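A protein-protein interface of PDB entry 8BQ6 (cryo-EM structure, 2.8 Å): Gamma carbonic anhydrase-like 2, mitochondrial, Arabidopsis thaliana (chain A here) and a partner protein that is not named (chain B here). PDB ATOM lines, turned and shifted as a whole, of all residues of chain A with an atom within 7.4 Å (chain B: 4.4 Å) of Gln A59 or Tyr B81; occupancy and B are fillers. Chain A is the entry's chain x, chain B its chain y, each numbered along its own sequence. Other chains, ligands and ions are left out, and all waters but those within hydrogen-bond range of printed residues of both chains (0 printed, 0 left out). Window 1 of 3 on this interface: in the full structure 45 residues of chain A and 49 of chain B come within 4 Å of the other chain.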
ATOM      1  N   ASP A  55       6.220 -11.654 -14.187  1.00  0.00           N
ATOM      2  CA  ASP A  55       6.732 -11.401 -12.845  1.00  0.00           C
ATOM      3  C   ASP A  55       7.656 -10.190 -12.915  1.00  0.00           C
ATOM      4  O   ASP A  55       8.693 -10.235 -13.582  1.00  0.00           O
ATOM      5  CB  ASP A  55       7.477 -12.625 -12.319  1.00  0.00           C
ATOM      6  CG  ASP A  55       7.723 -12.568 -10.824  1.00  0.00           C
ATOM      7  OD1 ASP A  55       7.846 -11.456 -10.273  1.00  0.00           O
ATOM      8  OD2 ASP A  55       7.842 -13.641 -10.201  1.00  0.00           O
ATOM      9  N   TYR A  56       7.289  -9.114 -12.214  1.00  0.00           N
ATOM     10  CA  TYR A  56       8.103  -7.904 -12.253  1.00  0.00           C
ATOM     11  C   TYR A  56       9.480  -8.109 -11.640  1.00  0.00           C
ATOM     12  O   TYR A  56      10.415  -7.386 -11.994  1.00  0.00           O
ATOM     13  CB  TYR A  56       7.389  -6.751 -11.545  1.00  0.00           C
ATOM     14  CG  TYR A  56       7.356  -6.867 -10.039  1.00  0.00           C
ATOM     15  CD1 TYR A  56       6.326  -7.539  -9.403  1.00  0.00           C
ATOM     16  CD2 TYR A  56       8.349  -6.298  -9.254  1.00  0.00           C
ATOM     17  CE1 TYR A  56       6.286  -7.647  -8.034  1.00  0.00           C
ATOM     18  CE2 TYR A  56       8.319  -6.403  -7.882  1.00  0.00           C
ATOM     19  CZ  TYR A  56       7.284  -7.079  -7.277  1.00  0.00           C
ATOM     20  OH  TYR A  56       7.241  -7.191  -5.908  1.00  0.00           O
ATOM     21  N   ARG A  57       9.625  -9.056 -10.714  1.00  0.00           N
ATOM     22  CA  ARG A  57      10.924  -9.305 -10.108  1.00  0.00           C
ATOM     23  C   ARG A  57      11.879 -10.032 -11.037  1.00  0.00           C
ATOM     24  O   ARG A  57      13.096  -9.941 -10.848  1.00  0.00           O
ATOM     25  CB  ARG A  57      10.751 -10.097  -8.814  1.00  0.00           C
ATOM     26  CG  ARG A  57       9.579  -9.608  -7.998  1.00  0.00           C
ATOM     27  CD  ARG A  57       9.185 -10.554  -6.894  1.00  0.00           C
ATOM     28  NE  ARG A  57       8.538 -11.765  -7.379  1.00  0.00           N
ATOM     29  CZ  ARG A  57       8.130 -12.750  -6.591  1.00  0.00           C
ATOM     30  NH1 ARG A  57       8.287 -12.691  -5.280  1.00  0.00           N
ATOM     31  NH2 ARG A  57       7.547 -13.815  -7.131  1.00  0.00           N
ATOM     32  N   GLY A  58      11.364 -10.734 -12.037  1.00  0.00           N
ATOM     33  CA  GLY A  58      12.196 -11.588 -12.856  1.00  0.00           C
ATOM     34  C   GLY A  58      12.560 -12.856 -12.106  1.00  0.00           C
ATOM     35  O   GLY A  58      12.029 -13.170 -11.043  1.00  0.00           O
ATOM     36  N   GLN A  59      13.494 -13.597 -12.686  1.00  0.00           N
ATOM     37  CA  GLN A  59      13.975 -14.823 -12.068  1.00  0.00           C
ATOM     38  C   GLN A  59      14.949 -14.480 -10.948  1.00  0.00           C
ATOM     39  O   GLN A  59      15.886 -13.701 -11.150  1.00  0.00           O
ATOM     40  CB  GLN A  59      14.643 -15.711 -13.112  1.00  0.00           C
ATOM     41  CG  GLN A  59      15.404 -16.878 -12.528  1.00  0.00           C
ATOM     42  CD  GLN A  59      14.485 -17.907 -11.924  1.00  0.00           C
ATOM     43  OE1 GLN A  59      13.610 -18.436 -12.601  1.00  0.00           O
ATOM     44  NE2 GLN A  59      14.681 -18.203 -10.648  1.00  0.00           N
ATOM     45  N   ARG A  60      14.728 -15.056  -9.771  1.00  0.00           N
ATOM     46  CA  ARG A  60      15.661 -14.879  -8.668  1.00  0.00           C
ATOM     47  C   ARG A  60      16.968 -15.602  -8.963  1.00  0.00           C
ATOM     48  O   ARG A  60      16.970 -16.759  -9.390  1.00  0.00           O
ATOM     49  CB  ARG A  60      15.044 -15.403  -7.375  1.00  0.00           C
ATOM     50  CG  ARG A  60      14.926 -14.364  -6.290  1.00  0.00           C
ATOM     51  CD  ARG A  60      14.645 -14.999  -4.950  1.00  0.00           C
ATOM     52  NE  ARG A  60      13.349 -15.664  -4.927  1.00  0.00           N
ATOM     53  CZ  ARG A  60      13.013 -16.613  -4.066  1.00  0.00           C
ATOM     54  NH1 ARG A  60      13.843 -17.007  -3.114  1.00  0.00           N
ATOM     55  NH2 ARG A  60      11.814 -17.178  -4.159  1.00  0.00           N
ATOM     56  N   GLN A  61      18.085 -14.908  -8.747  1.00  0.00           N
ATOM     57  CA  GLN A  61      19.384 -15.514  -9.007  1.00  0.00           C
ATOM     58  C   GLN A  61      19.689 -16.630  -8.015  1.00  0.00           C
ATOM     59  O   GLN A  61      20.222 -17.679  -8.397  1.00  0.00           O
ATOM     60  CB  GLN A  61      20.476 -14.451  -8.968  1.00  0.00           C
ATOM     61  CG  GLN A  61      21.858 -15.002  -9.211  1.00  0.00           C
ATOM     62  CD  GLN A  61      22.906 -13.921  -9.287  1.00  0.00           C
ATOM     63  OE1 GLN A  61      23.430 -13.472  -8.272  1.00  0.00           O
ATOM     64  NE2 GLN A  61      23.214 -13.493 -10.499  1.00  0.00           N
ATOM     65  N   ILE A  62      19.358 -16.427  -6.745  1.00  0.00           N
ATOM     66  CA  ILE A  62      19.663 -17.375  -5.680  1.00  0.00           C
ATOM     67  C   ILE A  62      18.362 -18.058  -5.293  1.00  0.00           C
ATOM     68  O   ILE A  62      17.430 -17.409  -4.804  1.00  0.00           O
ATOM     69  CB  ILE A  62      20.306 -16.685  -4.469  1.00  0.00           C
ATOM     70  CG1 ILE A  62      21.601 -15.972  -4.872  1.00  0.00           C
ATOM     71  CG2 ILE A  62      20.550 -17.685  -3.358  1.00  0.00           C
ATOM     72  CD1 ILE A  62      22.684 -16.887  -5.374  1.00  0.00           C
ATOM     73  N   ILE A  63      18.299 -19.369  -5.499  1.00  0.00           N
ATOM     74  CA  ILE A  63      17.109 -20.149  -5.171  1.00  0.00           C
ATOM     75  C   ILE A  63      17.456 -21.086  -4.021  1.00  0.00           C
ATOM     76  O   ILE A  63      18.032 -22.159  -4.247  1.00  0.00           O
ATOM     77  CB  ILE A  63      16.597 -20.929  -6.394  1.00  0.00           C
ATOM     78  CG1 ILE A  63      16.152 -19.970  -7.500  1.00  0.00           C
ATOM     79  CG2 ILE A  63      15.462 -21.868  -6.016  1.00  0.00           C
ATOM     80  CD1 ILE A  63      14.939 -19.149  -7.142  1.00  0.00           C
ATOM     81  N   LEU A  65      16.676 -23.938  -1.221  1.00  0.00           N
ATOM     82  CA  LEU A  65      15.785 -25.101  -1.197  1.00  0.00           C
ATOM     83  C   LEU A  65      15.833 -25.672   0.218  1.00  0.00           C
ATOM     84  O   LEU A  65      16.760 -26.402   0.573  1.00  0.00           O
ATOM     85  CB  LEU A  65      16.189 -26.134  -2.237  1.00  0.00           C
ATOM     86  CG  LEU A  65      16.002 -25.745  -3.705  1.00  0.00           C
ATOM     87  CD1 LEU A  65      16.680 -26.771  -4.583  1.00  0.00           C
ATOM     88  CD2 LEU A  65      14.534 -25.600  -4.075  1.00  0.00           C
ATOM     89  N   PRO A  80      24.227 -11.607 -13.696  1.00  0.00           N
ATOM     90  CA  PRO A  80      22.889 -11.349 -13.136  1.00  0.00           C
ATOM     91  C   PRO A  80      21.843 -12.396 -13.488  1.00  0.00           C
ATOM     92  O   PRO A  80      20.966 -12.669 -12.660  1.00  0.00           O
ATOM     93  CB  PRO A  80      22.536  -9.976 -13.717  1.00  0.00           C
ATOM     94  CG  PRO A  80      23.841  -9.332 -13.959  1.00  0.00           C
ATOM     95  CD  PRO A  80      24.775 -10.423 -14.378  1.00  0.00           C
ATOM     96  N   ASN A  81      21.894 -12.993 -14.677  1.00  0.00           N
ATOM     97  CA  ASN A  81      20.864 -13.946 -15.072  1.00  0.00           C
ATOM     98  C   ASN A  81      21.281 -15.401 -14.877  1.00  0.00           C
ATOM     99  O   ASN A  81      20.637 -16.298 -15.431  1.00  0.00           O
ATOM    100  CB  ASN A  81      20.429 -13.699 -16.521  1.00  0.00           C
ATOM    101  CG  ASN A  81      21.504 -14.040 -17.530  1.00  0.00           C
ATOM    102  OD1 ASN A  81      22.689 -14.081 -17.213  1.00  0.00           O
ATOM    103  ND2 ASN A  81      21.089 -14.271 -18.765  1.00  0.00           N
ATOM    104  N   VAL A  82      22.333 -15.654 -14.098  1.00  0.00           N
ATOM    105  CA  VAL A  82      22.653 -17.012 -13.681  1.00  0.00           C
ATOM    106  C   VAL A  82      21.646 -17.468 -12.629  1.00  0.00           C
ATOM    107  O   VAL A  82      21.162 -16.675 -11.813  1.00  0.00           O
ATOM    108  CB  VAL A  82      24.094 -17.068 -13.140  1.00  0.00           C
ATOM    109  CG1 VAL A  82      24.386 -18.392 -12.446  1.00  0.00           C
ATOM    110  CG2 VAL A  82      25.082 -16.819 -14.255  1.00  0.00           C
ATOM    111  N   VAL A  83      21.311 -18.755 -12.651  1.00  0.00           N
ATOM    112  CA  VAL A  83      20.461 -19.365 -11.636  1.00  0.00           C
ATOM    113  C   VAL A  83      21.311 -20.337 -10.830  1.00  0.00           C
ATOM    114  O   VAL A  83      21.871 -21.290 -11.383  1.00  0.00           O
ATOM    115  CB  VAL A  83      19.248 -20.075 -12.258  1.00  0.00           C
ATOM    116  CG1 VAL A  83      18.494 -20.866 -11.201  1.00  0.00           C
ATOM    117  CG2 VAL A  83      18.330 -19.065 -12.918  1.00  0.00           C
ATOM    118  N   LEU A  84      21.422 -20.086  -9.528  1.00  0.00           N
ATOM    119  CA  LEU A  84      22.054 -21.007  -8.591  1.00  0.00           C
ATOM    120  C   LEU A  84      20.979 -21.514  -7.644  1.00  0.00           C
ATOM    121  O   LEU A  84      20.307 -20.715  -6.986  1.00  0.00           O
ATOM    122  CB  LEU A  84      23.175 -20.333  -7.799  1.00  0.00           C
ATOM    123  CG  LEU A  84      24.258 -19.543  -8.528  1.00  0.00           C
ATOM    124  CD1 LEU A  84      25.134 -18.838  -7.517  1.00  0.00           C
ATOM    125  CD2 LEU A  84      25.088 -20.457  -9.404  1.00  0.00           C
ATOM    126  N   ALA A  85      20.818 -22.829  -7.568  1.00  0.00           N
ATOM    127  CA  ALA A  85      19.755 -23.405  -6.761  1.00  0.00           C
ATOM    128  C   ALA A  85      20.307 -24.503  -5.869  1.00  0.00           C
ATOM    129  O   ALA A  85      21.030 -25.387  -6.336  1.00  0.00           O
ATOM    130  CB  ALA A  85      18.632 -23.951  -7.645  1.00  0.00           C
ATOM    131  N   GLY A  99      23.686 -16.865 -18.546  1.00  0.00           N
ATOM    132  CA  GLY A  99      22.863 -17.964 -18.988  1.00  0.00           C
ATOM    133  C   GLY A  99      23.175 -19.304 -18.366  1.00  0.00           C
ATOM    134  O   GLY A  99      22.494 -20.283 -18.686  1.00  0.00           O
ATOM    135  N   ALA A 100      24.173 -19.387 -17.495  1.00  0.00           N
ATOM    136  CA  ALA A 100      24.517 -20.661 -16.886  1.00  0.00           C
ATOM    137  C   ALA A 100      23.530 -21.016 -15.782  1.00  0.00           C
ATOM    138  O   ALA A 100      22.978 -20.144 -15.106  1.00  0.00           O
ATOM    139  CB  ALA A 100      25.939 -20.627 -16.330  1.00  0.00           C
ATOM    140  N   VAL A 101      23.302 -22.316 -15.611  1.00  0.00           N
ATOM    141  CA  VAL A 101      22.413 -22.833 -14.577  1.00  0.00           C
ATOM    142  C   VAL A 101      23.190 -23.847 -13.754  1.00  0.00           C
ATOM    143  O   VAL A 101      23.801 -24.766 -14.310  1.00  0.00           O
ATOM    144  CB  VAL A 101      21.147 -23.477 -15.165  1.00  0.00           C
ATOM    145  CG1 VAL A 101      20.293 -24.071 -14.056  1.00  0.00           C
ATOM    146  CG2 VAL A 101      20.354 -22.460 -15.962  1.00  0.00           C
ATOM    147  N   LEU A 102      23.170 -23.678 -12.436  1.00  0.00           N
ATOM    148  CA  LEU A 102      23.814 -24.595 -11.503  1.00  0.00           C
ATOM    149  C   LEU A 102      22.765 -25.035 -10.497  1.00  0.00           C
ATOM    150  O   LEU A 102      22.393 -24.266  -9.605  1.00  0.00           O
ATOM    151  CB  LEU A 102      24.997 -23.936 -10.804  1.00  0.00           C
ATOM    152  CG  LEU A 102      26.232 -23.698 -11.662  1.00  0.00           C
ATOM    153  CD1 LEU A 102      26.069 -22.423 -12.447  1.00  0.00           C
ATOM    154  CD2 LEU A 102      27.429 -23.596 -10.761  1.00  0.00           C
ATOM    155  N   ARG A 103      22.289 -26.262 -10.642  1.00  0.00           N
ATOM    156  CA  ARG A 103      21.163 -26.763  -9.864  1.00  0.00           C
ATOM    157  C   ARG A 103      21.667 -27.874  -8.952  1.00  0.00           C
ATOM    158  O   ARG A 103      21.911 -28.996  -9.405  1.00  0.00           O
ATOM    159  CB  ARG A 103      20.054 -27.246 -10.791  1.00  0.00           C
ATOM    160  CG  ARG A 103      18.742 -27.522 -10.098  1.00  0.00           C
ATOM    161  CD  ARG A 103      17.572 -27.238 -11.013  1.00  0.00           C
ATOM    162  NE  ARG A 103      17.668 -27.976 -12.265  1.00  0.00           N
ATOM    163  CZ  ARG A 103      17.215 -29.208 -12.445  1.00  0.00           C
ATOM    164  NH1 ARG A 103      16.639 -29.883 -11.464  1.00  0.00           N
ATOM    165  NH2 ARG A 103      17.346 -29.779 -13.638  1.00  0.00           N
ATOM    166  N   ASP A 105      20.044 -29.626  -6.543  1.00  0.00           N
ATOM    167  CA  ASP A 105      18.913 -30.169  -5.803  1.00  0.00           C
ATOM    168  C   ASP A 105      19.042 -31.657  -5.504  1.00  0.00           C
ATOM    169  O   ASP A 105      18.347 -32.151  -4.614  1.00  0.00           O
ATOM    170  CB  ASP A 105      17.592 -29.909  -6.544  1.00  0.00           C
ATOM    171  CG  ASP A 105      17.679 -30.182  -8.031  1.00  0.00           C
ATOM    172  OD1 ASP A 105      18.644 -30.828  -8.480  1.00  0.00           O
ATOM    173  OD2 ASP A 105      16.758 -29.754  -8.755  1.00  0.00           O
ATOM    174  N   ARG A 120      26.100 -20.134 -20.640  1.00  0.00           N
ATOM    175  CA  ARG A 120      25.046 -21.092 -20.970  1.00  0.00           C
ATOM    176  C   ARG A 120      25.447 -22.534 -20.676  1.00  0.00           C
ATOM    177  O   ARG A 120      24.891 -23.467 -21.260  1.00  0.00           O
ATOM    178  CB  ARG A 120      24.599 -20.938 -22.429  1.00  0.00           C
ATOM    179  CG  ARG A 120      24.006 -19.566 -22.725  1.00  0.00           C
ATOM    180  CD  ARG A 120      22.990 -19.588 -23.850  1.00  0.00           C
ATOM    181  NE  ARG A 120      22.030 -20.679 -23.743  1.00  0.00           N
ATOM    182  CZ  ARG A 120      20.826 -20.568 -23.197  1.00  0.00           C
ATOM    183  NH1 ARG A 120      20.424 -19.442 -22.633  1.00  0.00           N
ATOM    184  NH2 ARG A 120      20.007 -21.615 -23.218  1.00  0.00           N
ATOM    185  N   VAL A 122      25.379 -25.791 -18.200  1.00  0.00           N
ATOM    186  CA  VAL A 122      24.445 -26.353 -17.234  1.00  0.00           C
ATOM    187  C   VAL A 122      25.201 -27.363 -16.392  1.00  0.00           C
ATOM    188  O   VAL A 122      25.788 -28.309 -16.929  1.00  0.00           O
ATOM    189  CB  VAL A 122      23.228 -27.001 -17.906  1.00  0.00           C
ATOM    190  CG1 VAL A 122      22.301 -27.579 -16.855  1.00  0.00           C
ATOM    191  CG2 VAL A 122      22.497 -25.985 -18.749  1.00  0.00           C
ATOM    192  N   PHE B  60       5.083 -26.815 -13.097  1.00  0.00           N
ATOM    193  CA  PHE B  60       6.136 -25.879 -12.737  1.00  0.00           C
ATOM    194  C   PHE B  60       6.638 -25.212 -14.008  1.00  0.00           C
ATOM    195  O   PHE B  60       7.077 -25.894 -14.938  1.00  0.00           O
ATOM    196  CB  PHE B  60       7.283 -26.583 -12.015  1.00  0.00           C
ATOM    197  CG  PHE B  60       8.500 -25.715 -11.811  1.00  0.00           C
ATOM    198  CD1 PHE B  60       8.377 -24.440 -11.286  1.00  0.00           C
ATOM    199  CD2 PHE B  60       9.761 -26.173 -12.150  1.00  0.00           C
ATOM    200  CE1 PHE B  60       9.484 -23.646 -11.096  1.00  0.00           C
ATOM    201  CE2 PHE B  60      10.871 -25.379 -11.965  1.00  0.00           C
ATOM    202  CZ  PHE B  60      10.732 -24.115 -11.435  1.00  0.00           C
ATOM    203  N   ALA B  62       9.455 -22.362 -14.646  1.00  0.00           N
ATOM    204  CA  ALA B  62      10.448 -21.474 -14.075  1.00  0.00           C
ATOM    205  C   ALA B  62      10.202 -20.052 -14.571  1.00  0.00           C
ATOM    206  O   ALA B  62       9.946 -19.848 -15.763  1.00  0.00           O
ATOM    207  CB  ALA B  62      11.855 -21.929 -14.457  1.00  0.00           C
ATOM    208  N   PRO B  63      10.265 -19.051 -13.691  1.00  0.00           N
ATOM    209  CA  PRO B  63      10.052 -17.668 -14.145  1.00  0.00           C
ATOM    210  C   PRO B  63      10.949 -17.275 -15.302  1.00  0.00           C
ATOM    211  O   PRO B  63      10.562 -16.433 -16.121  1.00  0.00           O
ATOM    212  CB  PRO B  63      10.350 -16.833 -12.893  1.00  0.00           C
ATOM    213  CG  PRO B  63      10.253 -17.770 -11.756  1.00  0.00           C
ATOM    214  CD  PRO B  63      10.549 -19.141 -12.251  1.00  0.00           C
ATOM    215  N   SER B  64      12.132 -17.875 -15.408  1.00  0.00           N
ATOM    216  CA  SER B  64      13.047 -17.561 -16.495  1.00  0.00           C
ATOM    217  C   SER B  64      12.721 -18.297 -17.786  1.00  0.00           C
ATOM    218  O   SER B  64      13.330 -17.998 -18.818  1.00  0.00           O
ATOM    219  CB  SER B  64      14.480 -17.878 -16.072  1.00  0.00           C
ATOM    220  OG  SER B  64      14.555 -19.156 -15.469  1.00  0.00           O
ATOM    221  N   TRP B  80      11.808 -25.924 -17.050  1.00  0.00           N
ATOM    222  CA  TRP B  80      12.848 -25.541 -16.113  1.00  0.00           C
ATOM    223  C   TRP B  80      13.556 -24.266 -16.569  1.00  0.00           C
ATOM    224  O   TRP B  80      13.223 -23.667 -17.594  1.00  0.00           O
ATOM    225  CB  TRP B  80      13.802 -26.718 -15.906  1.00  0.00           C
ATOM    226  CG  TRP B  80      13.158 -27.779 -15.063  1.00  0.00           C
ATOM    227  CD1 TRP B  80      12.300 -28.750 -15.482  1.00  0.00           C
ATOM    228  CD2 TRP B  80      13.285 -27.941 -13.647  1.00  0.00           C
ATOM    229  NE1 TRP B  80      11.894 -29.517 -14.419  1.00  0.00           N
ATOM    230  CE2 TRP B  80      12.488 -29.040 -13.280  1.00  0.00           C
ATOM    231  CE3 TRP B  80      14.005 -27.268 -12.655  1.00  0.00           C
ATOM    232  CZ2 TRP B  80      12.391 -29.483 -11.967  1.00  0.00           C
ATOM    233  CZ3 TRP B  80      13.909 -27.711 -11.356  1.00  0.00           C
ATOM    234  CH2 TRP B  80      13.107 -28.807 -11.021  1.00  0.00           C
ATOM    235  N   TYR B  81      14.527 -23.833 -15.766  1.00  0.00           N
ATOM    236  CA  TYR B  81      15.166 -22.536 -15.958  1.00  0.00           C
ATOM    237  C   TYR B  81      15.782 -22.413 -17.342  1.00  0.00           C
ATOM    238  O   TYR B  81      16.540 -23.280 -17.779  1.00  0.00           O
ATOM    239  CB  TYR B  81      16.241 -22.327 -14.898  1.00  0.00           C
ATOM    240  CG  TYR B  81      15.724 -22.498 -13.502  1.00  0.00           C
ATOM    241  CD1 TYR B  81      14.995 -21.495 -12.888  1.00  0.00           C
ATOM    242  CD2 TYR B  81      15.936 -23.677 -12.807  1.00  0.00           C
ATOM    243  CE1 TYR B  81      14.508 -21.650 -11.616  1.00  0.00           C
ATOM    244  CE2 TYR B  81      15.454 -23.840 -11.535  1.00  0.00           C
ATOM    245  CZ  TYR B  81      14.740 -22.825 -10.944  1.00  0.00           C
ATOM    246  OH  TYR B  81      14.256 -22.989  -9.672  1.00  0.00           O
ATOM    247  N   GLY B  82      15.463 -21.317 -18.022  1.00  0.00           N
ATOM    248  CA  GLY B  82      16.038 -21.027 -19.313  1.00  0.00           C
ATOM    249  C   GLY B  82      15.409 -21.740 -20.489  1.00  0.00           C
ATOM    250  O   GLY B  82      15.897 -21.582 -21.612  1.00  0.00           O
ATOM    251  N   CYS B  83      14.356 -22.522 -20.277  1.00  0.00           N
ATOM    252  CA  CYS B  83      13.720 -23.213 -21.387  1.00  0.00           C
ATOM    253  C   CYS B  83      12.923 -22.240 -22.243  1.00  0.00           C
ATOM    254  O   CYS B  83      12.293 -21.307 -21.741  1.00  0.00           O
ATOM    255  CB  CYS B  83      12.791 -24.312 -20.890  1.00  0.00           C
ATOM    256  SG  CYS B  83      13.587 -25.607 -19.968  1.00  0.00           S
ATOM    257  N   ASP B 102      16.665 -27.710 -18.030  1.00  0.00           N
ATOM    258  CA  ASP B 102      17.293 -26.375 -18.201  1.00  0.00           C
ATOM    259  C   ASP B 102      17.853 -26.034 -19.572  1.00  0.00           C
ATOM    260  O   ASP B 102      18.526 -26.898 -20.167  1.00  0.00           O
ATOM    261  CB  ASP B 102      18.426 -26.195 -17.183  1.00  0.00           C
ATOM    262  CG  ASP B 102      18.023 -26.531 -15.758  1.00  0.00           C
ATOM    263  OD1 ASP B 102      18.659 -27.423 -15.168  1.00  0.00           O
ATOM    264  OD2 ASP B 102      17.081 -25.893 -15.249  1.00  0.00           O
ATOM    265  N   ASN B 103      17.550 -24.820 -20.037  1.00  0.00           N
ATOM    266  CA  ASN B 103      18.169 -24.265 -21.239  1.00  0.00           C
ATOM    267  C   ASN B 103      17.789 -25.030 -22.507  1.00  0.00           C
ATOM    268  O   ASN B 103      18.493 -24.948 -23.516  1.00  0.00           O
ATOM    269  CB  ASN B 103      19.697 -24.203 -21.094  1.00  0.00           C
ATOM    270  CG  ASN B 103      20.161 -23.024 -20.257  1.00  0.00           C
ATOM    271  OD1 ASN B 103      19.355 -22.230 -19.782  1.00  0.00           O
ATOM    272  ND2 ASN B 103      21.468 -22.918 -20.058  1.00  0.00           N
ATOM    273  N   HIS B 214      10.801 -26.780  -6.350  1.00  0.00           N
ATOM    274  CA  HIS B 214      11.223 -25.599  -7.101  1.00  0.00           C
ATOM    275  C   HIS B 214      10.062 -24.632  -7.327  1.00  0.00           C
ATOM    276  O   HIS B 214      10.226 -23.413  -7.190  1.00  0.00           O
ATOM    277  CB  HIS B 214      11.858 -26.014  -8.421  1.00  0.00           C
ATOM    278  CG  HIS B 214      13.276 -26.469  -8.279  1.00  0.00           C
ATOM    279  ND1 HIS B 214      14.352 -25.631  -8.473  1.00  0.00           N
ATOM    280  CD2 HIS B 214      13.793 -27.672  -7.936  1.00  0.00           C
ATOM    281  CE1 HIS B 214      15.472 -26.301  -8.272  1.00  0.00           C
ATOM    282  NE2 HIS B 214      15.160 -27.543  -7.944  1.00  0.00           N
ATOM    283  N   ASN B 218       9.865 -20.721  -6.069  1.00  0.00           N
ATOM    284  CA  ASN B 218       9.867 -19.619  -7.027  1.00  0.00           C
ATOM    285  C   ASN B 218       8.627 -18.738  -6.926  1.00  0.00           C
ATOM    286  O   ASN B 218       8.650 -17.608  -7.423  1.00  0.00           O
ATOM    287  CB  ASN B 218      10.013 -20.161  -8.450  1.00  0.00           C
ATOM    288  CG  ASN B 218      11.451 -20.492  -8.798  1.00  0.00           C
ATOM    289  OD1 ASN B 218      12.217 -19.625  -9.214  1.00  0.00           O
ATOM    290  ND2 ASN B 218      11.827 -21.751  -8.622  1.00  0.00           N
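The side-chain amide oxygen (OE1) of Gln A59 sits at hydrogen-bond distance from the side-chain hydroxyl (OG) of Ser B64, at 3.1 Å. The side-chain amide oxygen (OD1) of Asn B218 lies within hydrogen-bond range of the side-chain amide nitrogen (NE2) of Gln A59 (3.2 Å). The backbone carbonyl oxygen (O) of Gly A99 lies within hydrogen-bond range of the side-chain amide nitrogen (ND2) of Asn B103 (3.1 Å). OD1 of Asp B102 is in salt-bridge range of NH2 of Arg A103. OD2 of Asp A105 is in hydrogen-bond range of NE2 of His B214 (2.8 Å).
OD1 of Asp A55 is in salt-bridge range of NE of Arg A57 (3.0 Å). The backbone NH (N) of Gly A99 sits at hydrogen-bond distance from the side-chain amide oxygen (OD1) of Asn A81. The backbone carbonyl oxygen (O) of Val A83 lies within hydrogen-bond range of the backbone NH (N) of Leu A102 (2.9 Å). N of Ala A85 is in hydrogen-bond range of O of Leu A102 (2.9 Å). The backbone carbonyl oxygen (O) of Tyr B81 sits at hydrogen-bond distance from the backbone NH (N) of Asn B103 (2.9 Å). OH of Tyr B81 lies within hydrogen-bond range of ND2 of Asn B218.
Among the printed residues, merely in contact across the chains: Gln A59 with Pro B63, Arg A120 with Asn B103, Gln A59 with Tyr B81, Ile A63 with Asn B218, Val A122 with Asn B103, Arg A103 with Trp B80, Arg A103 with His B214, Val A101 with Asp B102, Leu A65 with His B214, Val A83 with Tyr B81, Val A101 with Asn B103, Arg A57 with Asn B218 and Ala A85 with His B214.
Of chain B, only Pro B63 (3.2 Å), Ser B64 (3.1 Å), Tyr B81 (3.4 Å) and Asn B218 (3.2 Å) come within 4 Å of Gln A59. Printed residues of chain A within 4 Å of Tyr B81: Gln A59 and Val A83. Of the printed residues of chain A, Trp B80 touches Arg A103. Of the printed residues of chain B, Val A83 touches Tyr B81 (3.9 Å). Of the printed residues of chain B, Arg A120 touches Asn B103 (3.3 Å). Asn A81 touches none of the printed residues of chain B. The nearest residue of chain B that does not touch Gln A59 is Ala B62 (4.3 Å). The nearest printed residue of chain A that does not touch Tyr B81 is Ile A63 (4.01 Å). The nearest printed residue of chain B that does not touch Ala A85 is Tyr B81 (4.9 Å).
Of the 24 printed residues of chain A, 12 touch a printed residue of chain B. Hydrophobic or aromatic side chains of chain A that line the printed part of chain B: Ile A63, Leu A65, Val A83, Ala A85, Val A101 and Val A122. Among the printed residues, 18 pairs touch across the chains. Among the printed residues, Asp or Glu carboxylates within 4 Å of a Lys or Arg side-chain nitrogen of the other chain: Arg A103 with Asp B102.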
